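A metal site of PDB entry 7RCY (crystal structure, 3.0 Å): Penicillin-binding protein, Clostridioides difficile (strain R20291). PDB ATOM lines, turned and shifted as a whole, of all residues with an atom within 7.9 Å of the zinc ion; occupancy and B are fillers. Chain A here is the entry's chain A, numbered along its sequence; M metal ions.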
ATOM      1  N   ILE A 478      23.681  -3.408  14.859  1.00  0.00           N
ATOM      2  CA  ILE A 478      25.120  -3.833  14.875  1.00  0.00           C
ATOM      3  C   ILE A 478      25.166  -5.348  14.667  1.00  0.00           C
ATOM      4  O   ILE A 478      24.293  -6.039  15.220  1.00  0.00           O
ATOM      5  CB  ILE A 478      25.867  -3.419  16.169  1.00  0.00           C
ATOM      6  CG1 ILE A 478      25.349  -4.156  17.411  1.00  0.00           C
ATOM      7  CG2 ILE A 478      25.850  -1.909  16.337  1.00  0.00           C
ATOM      8  CD1 ILE A 478      26.083  -3.810  18.683  1.00  0.00           C
ATOM      9  N   ASN A 479      26.150  -5.814  13.899  1.00  0.00           N
ATOM     10  CA  ASN A 479      26.581  -7.240  13.878  1.00  0.00           C
ATOM     11  C   ASN A 479      27.209  -7.519  15.257  1.00  0.00           C
ATOM     12  O   ASN A 479      28.320  -7.007  15.532  1.00  0.00           O
ATOM     13  CB  ASN A 479      27.478  -7.556  12.674  1.00  0.00           C
ATOM     14  CG  ASN A 479      27.361  -8.991  12.206  1.00  0.00           C
ATOM     15  OD1 ASN A 479      28.359  -9.716  12.143  1.00  0.00           O
ATOM     16  ND2 ASN A 479      26.155  -9.433  11.882  1.00  0.00           N
ATOM     17  N   ASP A 480      26.479  -8.245  16.107  1.00  0.00           N
ATOM     18  CA  ASP A 480      26.809  -8.424  17.548  1.00  0.00           C
ATOM     19  C   ASP A 480      27.974  -9.414  17.656  1.00  0.00           C
ATOM     20  O   ASP A 480      27.782 -10.599  17.389  1.00  0.00           O
ATOM     21  CB  ASP A 480      25.574  -8.905  18.316  1.00  0.00           C
ATOM     22  CG  ASP A 480      25.800  -9.071  19.804  1.00  0.00           C
ATOM     23  OD1 ASP A 480      26.572  -8.282  20.373  1.00  0.00           O
ATOM     24  OD2 ASP A 480      25.192 -10.000  20.383  1.00  0.00           O
ATOM     25  N   PRO A 481      29.186  -8.964  18.051  1.00  0.00           N
ATOM     26  CA  PRO A 481      30.278  -9.879  18.376  1.00  0.00           C
ATOM     27  C   PRO A 481      29.998 -10.705  19.636  1.00  0.00           C
ATOM     28  O   PRO A 481      30.607 -11.744  19.790  1.00  0.00           O
ATOM     29  CB  PRO A 481      31.487  -8.971  18.633  1.00  0.00           C
ATOM     30  CG  PRO A 481      30.873  -7.645  19.035  1.00  0.00           C
ATOM     31  CD  PRO A 481      29.601  -7.556  18.211  1.00  0.00           C
ATOM     32  N   GLY A 482      29.123 -10.191  20.518  1.00  0.00           N
ATOM     33  CA  GLY A 482      28.736 -10.853  21.778  1.00  0.00           C
ATOM     34  C   GLY A 482      29.793 -10.730  22.843  1.00  0.00           C
ATOM     35  O   GLY A 482      29.566 -11.223  23.936  1.00  0.00           O
ATOM     36  N   VAL A 483      30.923 -10.092  22.530  1.00  0.00           N
ATOM     37  CA  VAL A 483      32.032  -9.884  23.510  1.00  0.00           C
ATOM     38  C   VAL A 483      32.855  -8.693  23.039  1.00  0.00           C
ATOM     39  O   VAL A 483      33.061  -8.548  21.823  1.00  0.00           O
ATOM     40  CB  VAL A 483      32.895 -11.141  23.676  1.00  0.00           C
ATOM     41  CG1 VAL A 483      33.555 -11.556  22.373  1.00  0.00           C
ATOM     42  CG2 VAL A 483      33.943 -10.972  24.758  1.00  0.00           C
ATOM     43  N   GLY A 492      31.127  -9.375  27.861  1.00  0.00           N
ATOM     44  CA  GLY A 492      30.369 -10.159  26.862  1.00  0.00           C
ATOM     45  C   GLY A 492      28.921 -10.417  27.263  1.00  0.00           C
ATOM     46  O   GLY A 492      28.627 -10.533  28.458  1.00  0.00           O
ATOM     47  N   ASP A 493      28.036 -10.548  26.270  1.00  0.00           N
ATOM     48  CA  ASP A 493      26.679 -11.114  26.481  1.00  0.00           C
ATOM     49  C   ASP A 493      26.869 -12.390  27.303  1.00  0.00           C
ATOM     50  O   ASP A 493      27.945 -12.998  27.209  1.00  0.00           O
ATOM     51  CB  ASP A 493      25.953 -11.382  25.155  1.00  0.00           C
ATOM     52  CG  ASP A 493      25.542 -10.141  24.376  1.00  0.00           C
ATOM     53  OD1 ASP A 493      25.651  -9.036  24.934  1.00  0.00           O
ATOM     54  OD2 ASP A 493      25.121 -10.281  23.211  1.00  0.00           O
ATOM     55  N   TYR A 494      25.866 -12.764  28.095  1.00  0.00           N
ATOM     56  CA  TYR A 494      25.812 -14.070  28.801  1.00  0.00           C
ATOM     57  C   TYR A 494      25.859 -15.166  27.726  1.00  0.00           C
ATOM     58  O   TYR A 494      26.520 -16.204  27.939  1.00  0.00           O
ATOM     59  CB  TYR A 494      24.578 -14.151  29.697  1.00  0.00           C
ATOM     60  CG  TYR A 494      24.189 -15.529  30.158  1.00  0.00           C
ATOM     61  CD1 TYR A 494      24.727 -16.081  31.320  1.00  0.00           C
ATOM     62  CD2 TYR A 494      23.278 -16.276  29.440  1.00  0.00           C
ATOM     63  CE1 TYR A 494      24.373 -17.344  31.750  1.00  0.00           C
ATOM     64  CE2 TYR A 494      22.906 -17.540  29.853  1.00  0.00           C
ATOM     65  CZ  TYR A 494      23.445 -18.076  31.011  1.00  0.00           C
ATOM     66  OH  TYR A 494      23.084 -19.327  31.411  1.00  0.00           O
ATOM     67  N   VAL A 495      25.230 -14.915  26.580  1.00  0.00           N
ATOM     68  CA  VAL A 495      25.123 -15.903  25.471  1.00  0.00           C
ATOM     69  C   VAL A 495      26.532 -16.212  24.916  1.00  0.00           C
ATOM     70  O   VAL A 495      26.691 -17.267  24.265  1.00  0.00           O
ATOM     71  CB  VAL A 495      24.157 -15.428  24.362  1.00  0.00           C
ATOM     72  CG1 VAL A 495      23.696 -16.597  23.503  1.00  0.00           C
ATOM     73  CG2 VAL A 495      22.949 -14.693  24.925  1.00  0.00           C
ATOM     74  N   TRP A 496      27.501 -15.318  25.166  1.00  0.00           N
ATOM     75  CA  TRP A 496      28.947 -15.532  24.863  1.00  0.00           C
ATOM     76  C   TRP A 496      29.612 -16.324  25.985  1.00  0.00           C
ATOM     77  O   TRP A 496      30.252 -17.332  25.670  1.00  0.00           O
ATOM     78  CB  TRP A 496      29.675 -14.198  24.664  1.00  0.00           C
ATOM     79  CG  TRP A 496      31.080 -14.346  24.167  1.00  0.00           C
ATOM     80  CD1 TRP A 496      31.489 -14.515  22.877  1.00  0.00           C
ATOM     81  CD2 TRP A 496      32.275 -14.338  24.970  1.00  0.00           C
ATOM     82  NE1 TRP A 496      32.850 -14.616  22.825  1.00  0.00           N
ATOM     83  CE2 TRP A 496      33.363 -14.499  24.091  1.00  0.00           C
ATOM     84  CE3 TRP A 496      32.530 -14.188  26.333  1.00  0.00           C
ATOM     85  CZ2 TRP A 496      34.684 -14.528  24.540  1.00  0.00           C
ATOM     86  CZ3 TRP A 496      33.830 -14.222  26.775  1.00  0.00           C
ATOM     87  CH2 TRP A 496      34.891 -14.382  25.890  1.00  0.00           C
ATOM     88  N   GLY A 501      28.735 -15.923  21.710  1.00  0.00           N
ATOM     89  CA  GLY A 501      27.880 -14.754  21.988  1.00  0.00           C
ATOM     90  C   GLY A 501      27.484 -14.048  20.714  1.00  0.00           C
ATOM     91  O   GLY A 501      28.303 -13.295  20.153  1.00  0.00           O
ATOM     92  N   ASN A 502      26.262 -14.276  20.245  1.00  0.00           N
ATOM     93  CA  ASN A 502      25.732 -13.501  19.103  1.00  0.00           C
ATOM     94  C   ASN A 502      24.227 -13.358  19.295  1.00  0.00           C
ATOM     95  O   ASN A 502      23.578 -14.376  19.571  1.00  0.00           O
ATOM     96  CB  ASN A 502      25.912 -14.268  17.790  1.00  0.00           C
ATOM     97  CG  ASN A 502      27.017 -13.690  16.943  1.00  0.00           C
ATOM     98  OD1 ASN A 502      26.954 -13.710  15.727  1.00  0.00           O
ATOM     99  ND2 ASN A 502      28.023 -13.141  17.611  1.00  0.00           N
ATOM    100  N   HIS A 503      23.732 -12.123  19.196  1.00  0.00           N
ATOM    101  CA  HIS A 503      22.315 -11.770  18.898  1.00  0.00           C
ATOM    102  C   HIS A 503      22.187 -11.358  17.417  1.00  0.00           C
ATOM    103  O   HIS A 503      21.210 -10.627  17.085  1.00  0.00           O
ATOM    104  CB  HIS A 503      21.837 -10.680  19.856  1.00  0.00           C
ATOM    105  CG  HIS A 503      21.740 -11.152  21.257  1.00  0.00           C
ATOM    106  ND1 HIS A 503      22.650 -10.773  22.229  1.00  0.00           N
ATOM    107  CD2 HIS A 503      20.878 -11.999  21.856  1.00  0.00           C
ATOM    108  CE1 HIS A 503      22.344 -11.356  23.365  1.00  0.00           C
ATOM    109  NE2 HIS A 503      21.254 -12.121  23.164  1.00  0.00           N
ATOM    110  N   GLY A 504      23.124 -11.800  16.570  1.00  0.00           N
ATOM    111  CA  GLY A 504      23.243 -11.431  15.141  1.00  0.00           C
ATOM    112  C   GLY A 504      23.138  -9.933  14.947  1.00  0.00           C
ATOM    113  O   GLY A 504      23.742  -9.199  15.743  1.00  0.00           O
ATOM    114  N   THR A 506      21.428  -6.450  15.304  1.00  0.00           N
ATOM    115  CA  THR A 506      20.809  -6.032  16.585  1.00  0.00           C
ATOM    116  C   THR A 506      20.588  -4.509  16.631  1.00  0.00           C
ATOM    117  O   THR A 506      21.580  -3.776  16.772  1.00  0.00           O
ATOM    118  CB  THR A 506      21.651  -6.547  17.758  1.00  0.00           C
ATOM    119  OG1 THR A 506      21.685  -7.966  17.667  1.00  0.00           O
ATOM    120  CG2 THR A 506      21.131  -6.128  19.118  1.00  0.00           C
ATOM    121  N   LYS A 510      15.777  -5.161  19.614  1.00  0.00           N
ATOM    122  CA  LYS A 510      16.272  -6.541  19.873  1.00  0.00           C
ATOM    123  C   LYS A 510      17.199  -6.541  21.110  1.00  0.00           C
ATOM    124  O   LYS A 510      17.117  -7.484  21.899  1.00  0.00           O
ATOM    125  CB  LYS A 510      16.960  -7.128  18.636  1.00  0.00           C
ATOM    126  CG  LYS A 510      17.268  -8.630  18.731  1.00  0.00           C
ATOM    127  CD  LYS A 510      18.234  -9.119  17.670  1.00  0.00           C
ATOM    128  CE  LYS A 510      17.670 -10.161  16.718  1.00  0.00           C
ATOM    129  NZ  LYS A 510      18.144 -11.523  17.080  1.00  0.00           N
ATOM    130  N   ALA A 511      18.023  -5.505  21.263  1.00  0.00           N
ATOM    131  CA  ALA A 511      18.910  -5.303  22.433  1.00  0.00           C
ATOM    132  C   ALA A 511      18.110  -5.354  23.735  1.00  0.00           C
ATOM    133  O   ALA A 511      18.403  -6.208  24.586  1.00  0.00           O
ATOM    134  CB  ALA A 511      19.636  -3.984  22.305  1.00  0.00           C
ATOM    135  N   GLU A 514      16.312  -9.162  23.871  1.00  0.00           N
ATOM    136  CA  GLU A 514      17.144 -10.345  24.262  1.00  0.00           C
ATOM    137  C   GLU A 514      18.187  -9.912  25.300  1.00  0.00           C
ATOM    138  O   GLU A 514      18.962 -10.761  25.767  1.00  0.00           O
ATOM    139  CB  GLU A 514      17.813 -10.983  23.032  1.00  0.00           C
ATOM    140  CG  GLU A 514      16.854 -11.612  22.029  1.00  0.00           C
ATOM    141  CD  GLU A 514      16.050 -12.815  22.511  1.00  0.00           C
ATOM    142  OE1 GLU A 514      16.543 -13.555  23.403  1.00  0.00           O
ATOM    143  OE2 GLU A 514      14.924 -13.023  22.007  1.00  0.00           O
ATOM    144  N   SER A 515      18.225  -8.627  25.663  1.00  0.00           N
ATOM    145  CA  SER A 515      19.161  -8.099  26.684  1.00  0.00           C
ATOM    146  C   SER A 515      20.605  -8.192  26.186  1.00  0.00           C
ATOM    147  O   SER A 515      21.405  -8.861  26.847  1.00  0.00           O
ATOM    148  CB  SER A 515      18.969  -8.828  27.995  1.00  0.00           C
ATOM    149  OG  SER A 515      19.680  -8.190  29.043  1.00  0.00           O
ATOM    150  N   CYS A 516      20.937  -7.515  25.086  1.00  0.00           N
ATOM    151  CA  CYS A 516      22.316  -7.431  24.527  1.00  0.00           C
ATOM    152  C   CYS A 516      23.118  -6.369  25.288  1.00  0.00           C
ATOM    153  O   CYS A 516      22.848  -5.172  25.082  1.00  0.00           O
ATOM    154  CB  CYS A 516      22.330  -7.075  23.045  1.00  0.00           C
ATOM    155  SG  CYS A 516      24.011  -7.004  22.363  1.00  0.00           S
ATOM    156  N   ASN A 517      24.105  -6.793  26.078  1.00  0.00           N
ATOM    157  CA  ASN A 517      24.951  -5.846  26.845  1.00  0.00           C
ATOM    158  C   ASN A 517      25.906  -5.141  25.884  1.00  0.00           C
ATOM    159  O   ASN A 517      26.330  -4.022  26.166  1.00  0.00           O
ATOM    160  CB  ASN A 517      25.787  -6.550  27.901  1.00  0.00           C
ATOM    161  CG  ASN A 517      25.002  -7.616  28.625  1.00  0.00           C
ATOM    162  OD1 ASN A 517      23.963  -8.043  28.137  1.00  0.00           O
ATOM    163  ND2 ASN A 517      25.482  -8.039  29.784  1.00  0.00           N
ATOM    164  N   ILE A 518      26.248  -5.809  24.786  1.00  0.00           N
ATOM    165  CA  ILE A 518      27.191  -5.241  23.784  1.00  0.00           C
ATOM    166  C   ILE A 518      26.571  -3.983  23.164  1.00  0.00           C
ATOM    167  O   ILE A 518      27.292  -2.987  23.019  1.00  0.00           O
ATOM    168  CB  ILE A 518      27.541  -6.299  22.720  1.00  0.00           C
ATOM    169  CG1 ILE A 518      28.088  -7.600  23.327  1.00  0.00           C
ATOM    170  CG2 ILE A 518      28.474  -5.718  21.667  1.00  0.00           C
ATOM    171  CD1 ILE A 518      29.042  -7.413  24.484  1.00  0.00           C
ATOM    172  N   TYR A 519      25.286  -4.040  22.831  1.00  0.00           N
ATOM    173  CA  TYR A 519      24.538  -2.893  22.244  1.00  0.00           C
ATOM    174  C   TYR A 519      24.526  -1.733  23.243  1.00  0.00           C
ATOM    175  O   TYR A 519      24.714  -0.584  22.813  1.00  0.00           O
ATOM    176  CB  TYR A 519      23.102  -3.278  21.890  1.00  0.00           C
ATOM    177  CG  TYR A 519      22.362  -2.205  21.116  1.00  0.00           C
ATOM    178  CD1 TYR A 519      21.762  -1.144  21.765  1.00  0.00           C
ATOM    179  CD2 TYR A 519      22.276  -2.263  19.732  1.00  0.00           C
ATOM    180  CE1 TYR A 519      21.089  -0.159  21.058  1.00  0.00           C
ATOM    181  CE2 TYR A 519      21.599  -1.280  19.013  1.00  0.00           C
ATOM    182  CZ  TYR A 519      21.001  -0.233  19.678  1.00  0.00           C
ATOM    183  OH  TYR A 519      20.332   0.737  18.989  1.00  0.00           O
ATOM    184  N   MET A 520      24.312  -2.042  24.519  1.00  0.00           N
ATOM    185  CA  MET A 520      24.186  -1.030  25.605  1.00  0.00           C
ATOM    186  C   MET A 520      25.557  -0.407  25.879  1.00  0.00           C
ATOM    187  O   MET A 520      25.627   0.834  26.019  1.00  0.00           O
ATOM    188  CB  MET A 520      23.611  -1.656  26.870  1.00  0.00           C
ATOM    189  CG  MET A 520      22.184  -2.136  26.690  1.00  0.00           C
ATOM    190  SD  MET A 520      20.994  -0.788  26.384  1.00  0.00           S
ATOM    191  CE  MET A 520      19.607  -1.710  25.743  1.00  0.00           C
HETATM  192 ZN    ZN M   1      24.033  -9.297  22.048  1.00  0.00          ZN
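The zinc ion is bound by OD2 of Asp 493 (1.9 Å), ND1 of His 503 (2.0 Å), OD2 of Asp 480 (2.1 Å) and SG of Cys 516 (2.3 Å).
The backbone NH of Asp 480 lies within hydrogen-bond range of the backbone carbonyl oxygen of Gly 504, 2.9 Å away. O of Asp 480 lies within hydrogen-bond range of ND2 of Asn 502, 2.6 Å away. The backbone NH of Ile 518 lies close to the side-chain carboxylate of Asp 493. N of Tyr 519 sits close to SG of Cys 516 (3.3 Å). The side-chain amino group of Lys 510 sits at hydrogen-bond distance from the backbone carbonyl oxygen of His 503 (3.2 Å). The backbone carbonyl oxygen (O) of His 503 is in hydrogen-bond range of the side-chain hydroxyl (OG1) of Thr 506, 2.8 Å away. The side-chain carboxylate (OD1) of Asp 493 sits at hydrogen-bond distance from the backbone NH (N) of Asn 517, 3.0 Å away. N of Asp 493 is in hydrogen-bond range of O of Gly 482, 2.9 Å away.
Four residues have an atom within 4 Å of the zinc ion: Asp 480, Asp 493, His 503 and Cys 516. The nearest printed residue that does not touch the zinc ion is Ile 518 (4.6 Å).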
